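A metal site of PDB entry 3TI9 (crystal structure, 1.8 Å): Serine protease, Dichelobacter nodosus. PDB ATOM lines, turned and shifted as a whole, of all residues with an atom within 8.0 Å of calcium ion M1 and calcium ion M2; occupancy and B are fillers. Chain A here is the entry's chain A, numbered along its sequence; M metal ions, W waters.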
ATOM      1  N   TYR A  58     -20.871 -21.205 -18.793  1.00  0.00           N
ATOM      2  CA  TYR A  58     -20.514 -20.552 -20.049  1.00  0.00           C
ATOM      3  C   TYR A  58     -21.490 -20.910 -21.159  1.00  0.00           C
ATOM      4  O   TYR A  58     -22.046 -22.003 -21.185  1.00  0.00           O
ATOM      5  CB  TYR A  58     -19.075 -20.879 -20.472  1.00  0.00           C
ATOM      6  CG  TYR A  58     -18.455 -19.754 -21.286  1.00  0.00           C
ATOM      7  CD1 TYR A  58     -17.878 -18.655 -20.666  1.00  0.00           C
ATOM      8  CD2 TYR A  58     -18.481 -19.784 -22.676  1.00  0.00           C
ATOM      9  CE1 TYR A  58     -17.334 -17.603 -21.397  1.00  0.00           C
ATOM     10  CE2 TYR A  58     -17.933 -18.739 -23.438  1.00  0.00           C
ATOM     11  CZ  TYR A  58     -17.364 -17.656 -22.779  1.00  0.00           C
ATOM     12  OH  TYR A  58     -16.824 -16.627 -23.503  1.00  0.00           O
ATOM     13  N   ASP A  59     -21.701 -19.958 -22.077  1.00  0.00           N
ATOM     14  CA  ASP A  59     -22.596 -20.132 -23.218  1.00  0.00           C
ATOM     15  C   ASP A  59     -21.748 -20.379 -24.450  1.00  0.00           C
ATOM     16  O   ASP A  59     -21.131 -19.458 -25.001  1.00  0.00           O
ATOM     17  CB  ASP A  59     -23.469 -18.884 -23.387  1.00  0.00           C
ATOM     18  CG  ASP A  59     -24.633 -19.093 -24.346  1.00  0.00           C
ATOM     19  OD1 ASP A  59     -24.533 -19.922 -25.298  1.00  0.00           O
ATOM     20  OD2 ASP A  59     -25.650 -18.394 -24.160  1.00  0.00           O
ATOM     21  N   PHE A  60     -21.733 -21.626 -24.901  1.00  0.00           N
ATOM     22  CA  PHE A  60     -20.947 -22.025 -26.068  1.00  0.00           C
ATOM     23  C   PHE A  60     -21.695 -21.926 -27.401  1.00  0.00           C
ATOM     24  O   PHE A  60     -21.114 -22.220 -28.452  1.00  0.00           O
ATOM     25  CB  PHE A  60     -20.376 -23.422 -25.859  1.00  0.00           C
ATOM     26  CG  PHE A  60     -19.179 -23.450 -24.952  1.00  0.00           C
ATOM     27  CD1 PHE A  60     -17.895 -23.354 -25.479  1.00  0.00           C
ATOM     28  CD2 PHE A  60     -19.330 -23.526 -23.566  1.00  0.00           C
ATOM     29  CE1 PHE A  60     -16.784 -23.360 -24.642  1.00  0.00           C
ATOM     30  CE2 PHE A  60     -18.222 -23.524 -22.718  1.00  0.00           C
ATOM     31  CZ  PHE A  60     -16.945 -23.438 -23.266  1.00  0.00           C
ATOM     32  N   ILE A  61     -22.956 -21.497 -27.386  1.00  0.00           N
ATOM     33  CA  ILE A  61     -23.711 -21.355 -28.634  1.00  0.00           C
ATOM     34  C   ILE A  61     -23.062 -20.248 -29.499  1.00  0.00           C
ATOM     35  O   ILE A  61     -23.026 -19.085 -29.105  1.00  0.00           O
ATOM     36  CB  ILE A  61     -25.227 -21.117 -28.412  1.00  0.00           C
ATOM     37  CG1 ILE A  61     -25.820 -22.211 -27.505  1.00  0.00           C
ATOM     38  CG2 ILE A  61     -25.967 -21.077 -29.760  1.00  0.00           C
ATOM     39  CD1 ILE A  61     -27.258 -21.932 -27.006  1.00  0.00           C
ATOM     40  N   SER A  62     -22.532 -20.663 -30.663  1.00  0.00           N
ATOM     41  CA  SER A  62     -21.803 -19.779 -31.568  1.00  0.00           C
ATOM     42  C   SER A  62     -22.713 -18.880 -32.425  1.00  0.00           C
ATOM     43  O   SER A  62     -22.284 -17.805 -32.865  1.00  0.00           O
ATOM     44  CB  SER A  62     -20.883 -20.590 -32.480  1.00  0.00           C
ATOM     45  OG  SER A  62     -19.889 -21.266 -31.720  1.00  0.00           O
ATOM     46  N   SER A  63     -23.945 -19.334 -32.645  1.00  0.00           N
ATOM     47  CA  SER A  63     -24.914 -18.596 -33.438  1.00  0.00           C
ATOM     48  C   SER A  63     -25.748 -17.683 -32.544  1.00  0.00           C
ATOM     49  O   SER A  63     -26.485 -18.156 -31.681  1.00  0.00           O
ATOM     50  CB  SER A  63     -25.840 -19.561 -34.174  1.00  0.00           C
ATOM     51  OG  SER A  63     -27.023 -18.900 -34.597  1.00  0.00           O
ATOM     52  N   ALA A  64     -25.631 -16.377 -32.768  1.00  0.00           N
ATOM     53  CA  ALA A  64     -26.408 -15.393 -32.006  1.00  0.00           C
ATOM     54  C   ALA A  64     -27.935 -15.579 -32.137  1.00  0.00           C
ATOM     55  O   ALA A  64     -28.625 -15.578 -31.116  1.00  0.00           O
ATOM     56  CB  ALA A  64     -26.006 -13.965 -32.383  1.00  0.00           C
ATOM     57  N   PRO A  65     -28.461 -15.745 -33.379  1.00  0.00           N
ATOM     58  CA  PRO A  65     -29.906 -15.957 -33.521  1.00  0.00           C
ATOM     59  C   PRO A  65     -30.420 -17.181 -32.765  1.00  0.00           C
ATOM     60  O   PRO A  65     -31.490 -17.133 -32.170  1.00  0.00           O
ATOM     61  CB  PRO A  65     -30.089 -16.139 -35.039  1.00  0.00           C
ATOM     62  CG  PRO A  65     -28.915 -15.461 -35.643  1.00  0.00           C
ATOM     63  CD  PRO A  65     -27.787 -15.713 -34.699  1.00  0.00           C
ATOM     64  N   LYS A  66     -29.648 -18.275 -32.783  1.00  0.00           N
ATOM     65  CA  LYS A  66     -30.043 -19.497 -32.105  1.00  0.00           C
ATOM     66  C   LYS A  66     -29.949 -19.406 -30.577  1.00  0.00           C
ATOM     67  O   LYS A  66     -30.707 -20.061 -29.852  1.00  0.00           O
ATOM     68  CB  LYS A  66     -29.254 -20.697 -32.646  1.00  0.00           C
ATOM     69  CG  LYS A  66     -29.690 -21.061 -34.067  1.00  0.00           C
ATOM     70  CD  LYS A  66     -29.023 -22.311 -34.585  1.00  0.00           C
ATOM     71  CE  LYS A  66     -29.605 -22.683 -35.949  1.00  0.00           C
ATOM     72  NZ  LYS A  66     -28.819 -23.743 -36.648  1.00  0.00           N
ATOM     73  N   ALA A  67     -29.025 -18.565 -30.095  1.00  0.00           N
ATOM     74  CA  ALA A  67     -28.858 -18.317 -28.661  1.00  0.00           C
ATOM     75  C   ALA A  67     -29.859 -17.321 -28.094  1.00  0.00           C
ATOM     76  O   ALA A  67     -30.060 -17.272 -26.878  1.00  0.00           O
ATOM     77  CB  ALA A  67     -27.424 -17.848 -28.385  1.00  0.00           C
ATOM     78  N   ARG A  68     -30.476 -16.519 -28.975  1.00  0.00           N
ATOM     79  CA  ARG A  68     -31.515 -15.539 -28.601  1.00  0.00           C
ATOM     80  C   ARG A  68     -31.049 -14.524 -27.539  1.00  0.00           C
ATOM     81  O   ARG A  68     -31.851 -14.090 -26.700  1.00  0.00           O
ATOM     82  CB  ARG A  68     -32.807 -16.249 -28.163  1.00  0.00           C
ATOM     83  CG  ARG A  68     -33.586 -16.869 -29.315  1.00  0.00           C
ATOM     84  CD  ARG A  68     -34.807 -17.586 -28.796  1.00  0.00           C
ATOM     85  NE  ARG A  68     -35.812 -17.791 -29.842  1.00  0.00           N
ATOM     86  CZ  ARG A  68     -36.384 -18.960 -30.127  1.00  0.00           C
ATOM     87  NH1 ARG A  68     -36.071 -20.068 -29.463  1.00  0.00           N
ATOM     88  NH2 ARG A  68     -37.297 -18.997 -31.094  1.00  0.00           N
ATOM     89  N   ASP A  69     -29.777 -14.159 -27.587  1.00  0.00           N
ATOM     90  CA  ASP A  69     -29.192 -13.249 -26.603  1.00  0.00           C
ATOM     91  C   ASP A  69     -28.345 -12.143 -27.233  1.00  0.00           C
ATOM     92  O   ASP A  69     -27.612 -11.433 -26.546  1.00  0.00           O
ATOM     93  CB  ASP A  69     -28.387 -14.040 -25.557  1.00  0.00           C
ATOM     94  CG  ASP A  69     -27.245 -14.810 -26.160  1.00  0.00           C
ATOM     95  OD1 ASP A  69     -26.942 -14.609 -27.360  1.00  0.00           O
ATOM     96  OD2 ASP A  69     -26.624 -15.628 -25.442  1.00  0.00           O
ATOM     97  N   GLY A  70     -28.431 -12.020 -28.559  1.00  0.00           N
ATOM     98  CA  GLY A  70     -27.798 -10.918 -29.294  1.00  0.00           C
ATOM     99  C   GLY A  70     -26.296 -11.001 -29.532  1.00  0.00           C
ATOM    100  O   GLY A  70     -25.717 -10.116 -30.158  1.00  0.00           O
ATOM    101  N   ASP A  71     -25.652 -12.066 -29.038  1.00  0.00           N
ATOM    102  CA  ASP A  71     -24.223 -12.255 -29.277  1.00  0.00           C
ATOM    103  C   ASP A  71     -23.830 -13.723 -29.480  1.00  0.00           C
ATOM    104  O   ASP A  71     -24.654 -14.622 -29.303  1.00  0.00           O
ATOM    105  CB  ASP A  71     -23.355 -11.571 -28.188  1.00  0.00           C
ATOM    106  CG  ASP A  71     -23.589 -12.136 -26.791  1.00  0.00           C
ATOM    107  OD1 ASP A  71     -24.261 -13.187 -26.625  1.00  0.00           O
ATOM    108  OD2 ASP A  71     -23.091 -11.522 -25.827  1.00  0.00           O
ATOM    109  N   GLN A  72     -22.579 -13.955 -29.848  1.00  0.00           N
ATOM    110  CA  GLN A  72     -22.086 -15.310 -30.028  1.00  0.00           C
ATOM    111  C   GLN A  72     -21.724 -15.899 -28.661  1.00  0.00           C
ATOM    112  O   GLN A  72     -22.482 -15.737 -27.686  1.00  0.00           O
ATOM    113  CB  GLN A  72     -20.926 -15.347 -31.023  1.00  0.00           C
ATOM    114  CG  GLN A  72     -21.302 -14.875 -32.422  1.00  0.00           C
ATOM    115  CD  GLN A  72     -20.195 -15.116 -33.427  1.00  0.00           C
ATOM    116  OE1 GLN A  72     -19.244 -14.343 -33.513  1.00  0.00           O
ATOM    117  NE2 GLN A  72     -20.325 -16.179 -34.205  1.00  0.00           N
ATOM    118  N   ARG A  73     -20.593 -16.580 -28.542  1.00  0.00           N
ATOM    119  CA  ARG A  73     -20.233 -17.183 -27.256  1.00  0.00           C
ATOM    120  C   ARG A  73     -20.058 -16.111 -26.194  1.00  0.00           C
ATOM    121  O   ARG A  73     -19.549 -15.015 -26.480  1.00  0.00           O
ATOM    122  CB  ARG A  73     -19.001 -18.083 -27.387  1.00  0.00           C
ATOM    123  CG  ARG A  73     -19.259 -19.338 -28.216  1.00  0.00           C
ATOM    124  CD  ARG A  73     -18.032 -20.239 -28.247  1.00  0.00           C
ATOM    125  NE  ARG A  73     -18.339 -21.540 -28.840  1.00  0.00           N
ATOM    126  CZ  ARG A  73     -17.435 -22.479 -29.083  1.00  0.00           C
ATOM    127  NH1 ARG A  73     -16.154 -22.268 -28.794  1.00  0.00           N
ATOM    128  NH2 ARG A  73     -17.810 -23.638 -29.624  1.00  0.00           N
ATOM    129  N   ASP A  74     -20.521 -16.404 -24.986  1.00  0.00           N
ATOM    130  CA  ASP A  74     -20.536 -15.436 -23.879  1.00  0.00           C
ATOM    131  C   ASP A  74     -20.560 -16.133 -22.519  1.00  0.00           C
ATOM    132  O   ASP A  74     -20.792 -17.347 -22.430  1.00  0.00           O
ATOM    133  CB  ASP A  74     -21.743 -14.504 -24.015  1.00  0.00           C
ATOM    134  CG  ASP A  74     -23.050 -15.232 -23.791  1.00  0.00           C
ATOM    135  OD1 ASP A  74     -23.707 -15.629 -24.778  1.00  0.00           O
ATOM    136  OD2 ASP A  74     -23.431 -15.412 -22.621  1.00  0.00           O
ATOM    137  N   ASN A  75     -20.344 -15.364 -21.456  1.00  0.00           N
ATOM    138  CA  ASN A  75     -20.235 -15.914 -20.100  1.00  0.00           C
ATOM    139  C   ASN A  75     -21.549 -16.021 -19.324  1.00  0.00           C
ATOM    140  O   ASN A  75     -21.529 -16.187 -18.103  1.00  0.00           O
ATOM    141  CB  ASN A  75     -19.198 -15.120 -19.298  1.00  0.00           C
ATOM    142  CG  ASN A  75     -19.587 -13.658 -19.136  1.00  0.00           C
ATOM    143  OD1 ASN A  75     -20.751 -13.278 -19.295  1.00  0.00           O
ATOM    144  ND2 ASN A  75     -18.603 -12.817 -18.813  1.00  0.00           N
ATOM    145  N   ASN A  76     -22.672 -15.894 -20.029  1.00  0.00           N
ATOM    146  CA  ASN A  76     -23.995 -15.979 -19.411  1.00  0.00           C
ATOM    147  C   ASN A  76     -24.793 -17.149 -19.993  1.00  0.00           C
ATOM    148  O   ASN A  76     -25.444 -17.004 -21.038  1.00  0.00           O
ATOM    149  CB  ASN A  76     -24.764 -14.655 -19.602  1.00  0.00           C
ATOM    150  CG  ASN A  76     -26.144 -14.668 -18.919  1.00  0.00           C
ATOM    151  OD1 ASN A  76     -26.492 -15.606 -18.202  1.00  0.00           O
ATOM    152  ND2 ASN A  76     -26.929 -13.629 -19.157  1.00  0.00           N
ATOM    153  N   PRO A  77     -24.744 -18.317 -19.330  1.00  0.00           N
ATOM    154  CA  PRO A  77     -25.458 -19.500 -19.831  1.00  0.00           C
ATOM    155  C   PRO A  77     -26.966 -19.475 -19.549  1.00  0.00           C
ATOM    156  O   PRO A  77     -27.575 -20.531 -19.361  1.00  0.00           O
ATOM    157  CB  PRO A  77     -24.784 -20.642 -19.072  1.00  0.00           C
ATOM    158  CG  PRO A  77     -24.441 -20.026 -17.740  1.00  0.00           C
ATOM    159  CD  PRO A  77     -24.019 -18.605 -18.077  1.00  0.00           C
ATOM    160  N   ALA A  78     -27.587 -18.291 -19.548  1.00  0.00           N
ATOM    161  CA  ALA A  78     -29.031 -18.217 -19.361  1.00  0.00           C
ATOM    162  C   ALA A  78     -29.772 -18.931 -20.500  1.00  0.00           C
ATOM    163  O   ALA A  78     -29.442 -18.756 -21.672  1.00  0.00           O
ATOM    164  CB  ALA A  78     -29.498 -16.763 -19.261  1.00  0.00           C
ATOM    165  N   ASP A  79     -30.740 -19.767 -20.128  1.00  0.00           N
ATOM    166  CA  ASP A  79     -31.626 -20.370 -21.129  1.00  0.00           C
ATOM    167  C   ASP A  79     -32.693 -19.339 -21.535  1.00  0.00           C
ATOM    168  O   ASP A  79     -33.562 -18.985 -20.745  1.00  0.00           O
ATOM    169  CB  ASP A  79     -32.277 -21.658 -20.603  1.00  0.00           C
ATOM    170  CG  ASP A  79     -32.992 -22.462 -21.701  1.00  0.00           C
ATOM    171  OD1 ASP A  79     -33.088 -21.989 -22.853  1.00  0.00           O
ATOM    172  OD2 ASP A  79     -33.467 -23.571 -21.385  1.00  0.00           O
ATOM    173  N   GLU A  80     -32.588 -18.859 -22.783  1.00  0.00           N
ATOM    174  CA  GLU A  80     -33.514 -17.857 -23.319  1.00  0.00           C
ATOM    175  C   GLU A  80     -34.776 -18.498 -23.899  1.00  0.00           C
ATOM    176  O   GLU A  80     -35.709 -17.802 -24.324  1.00  0.00           O
ATOM    177  CB  GLU A  80     -32.817 -17.010 -24.398  1.00  0.00           C
ATOM    178  CG  GLU A  80     -31.422 -16.499 -24.018  1.00  0.00           C
ATOM    179  CD  GLU A  80     -31.436 -15.423 -22.941  1.00  0.00           C
ATOM    180  OE1 GLU A  80     -32.537 -14.921 -22.604  1.00  0.00           O
ATOM    181  OE2 GLU A  80     -30.332 -15.076 -22.442  1.00  0.00           O
ATOM    182  N   ARG A 136     -24.042 -24.057 -21.535  1.00  0.00           N
ATOM    183  CA  ARG A 136     -25.092 -23.912 -22.548  1.00  0.00           C
ATOM    184  C   ARG A 136     -24.563 -24.180 -23.950  1.00  0.00           C
ATOM    185  O   ARG A 136     -23.675 -23.473 -24.446  1.00  0.00           O
ATOM    186  CB  ARG A 136     -25.738 -22.523 -22.448  1.00  0.00           C
ATOM    187  CG  ARG A 136     -26.971 -22.382 -23.345  1.00  0.00           C
ATOM    188  CD  ARG A 136     -27.535 -20.971 -23.332  1.00  0.00           C
ATOM    189  NE  ARG A 136     -28.841 -20.904 -23.996  1.00  0.00           N
ATOM    190  CZ  ARG A 136     -29.278 -19.862 -24.709  1.00  0.00           C
ATOM    191  NH1 ARG A 136     -28.513 -18.800 -24.902  1.00  0.00           N
ATOM    192  NH2 ARG A 136     -30.494 -19.905 -25.241  1.00  0.00           N
HETATM  193 CA    CA M   1     -24.634 -15.489 -26.954  1.00  0.00          CA
HETATM  194 CA    CA M   2     -25.764 -16.139 -23.232  1.00  0.00          CA
HETATM  195  O   HOH W   1     -28.090 -16.496 -22.672  1.00  0.00           O
HETATM  196  O   HOH W   2     -24.480 -17.868 -27.300  1.00  0.00           O
HETATM  197  O   HOH W   3     -26.084 -13.825 -22.725  1.00  0.00           O
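The side-chain amide nitrogen (NE2) of Gln 72 lies within hydrogen-bond range of the backbone carbonyl oxygen (O) of Ser 62 (2.9 Å).
The side-chain carboxylate (OD1) of Asp 59 lies within hydrogen-bond range of the backbone NH (N) of Ile 61.
The guanidinium group (NH1) of Arg 136 sits close to the side-chain carboxylate (OD2) of Asp 59, 3.0 Å away.
N of Ala 78 sits close to OD1 of Asn 76, at 3.2 Å.
NH1 of Arg 136 sits close to OD2 of Asp 69, at 3.7 Å.
The backbone carbonyl oxygen (O) of Ala 67 sits at hydrogen-bond distance from the guanidinium group (NH1) of Arg 136.
Ala 67 touches calcium ion M1 (CB to CA, 3.9 Å).
Five residues have an atom within 4 Å of calcium ion M1: Ala 67, Asp 69, Asp 71, Gln 72 and Asp 74.
Within 4 Å of calcium ion M2: Asp 59, Asp 69, Asp 74 and Asn 76.
The nearest printed residue that does not touch calcium ion M2 is Arg 136 (4.2 Å).
Calcium ion M1 is bound by the backbone carbonyl oxygen (O) of Gln 72 (2.3 Å), the side-chain carboxylate (OD1) of Asp 71 (2.4 Å), the side-chain carboxylate (OD1) of Asp 74 (2.4 Å), water W2 (2.4 Å), the side-chain carboxylate (OD1) of Asp 69 (2.5 Å), the side-chain carboxylate (OD2) of Asp 69 (2.5 Å) and the backbone carbonyl oxygen (O) of Asp 71 (2.5 Å).
Calcium ion M2 is bound by the backbone carbonyl oxygen (O) of Asn 76, water W3, water W1, the side-chain carboxylate (OD2) of Asp 69, the side-chain carboxylate (OD2) of Asp 59, the side-chain carboxylate (OD2) of Asp 74 and the side-chain carboxylate (OD1) of Asp 74.
Calcium ion M2 has seven donor atoms within binding distance.
Water W2 lies within hydrogen-bond range of O of Ile 61 and OD1 of Asp 59.
Water W1 lies within hydrogen-bond range of OE2 of Glu 80 (2.7 Å), O of Ala 78 (2.8 Å) and NH1 of Arg 136 (3.2 Å).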
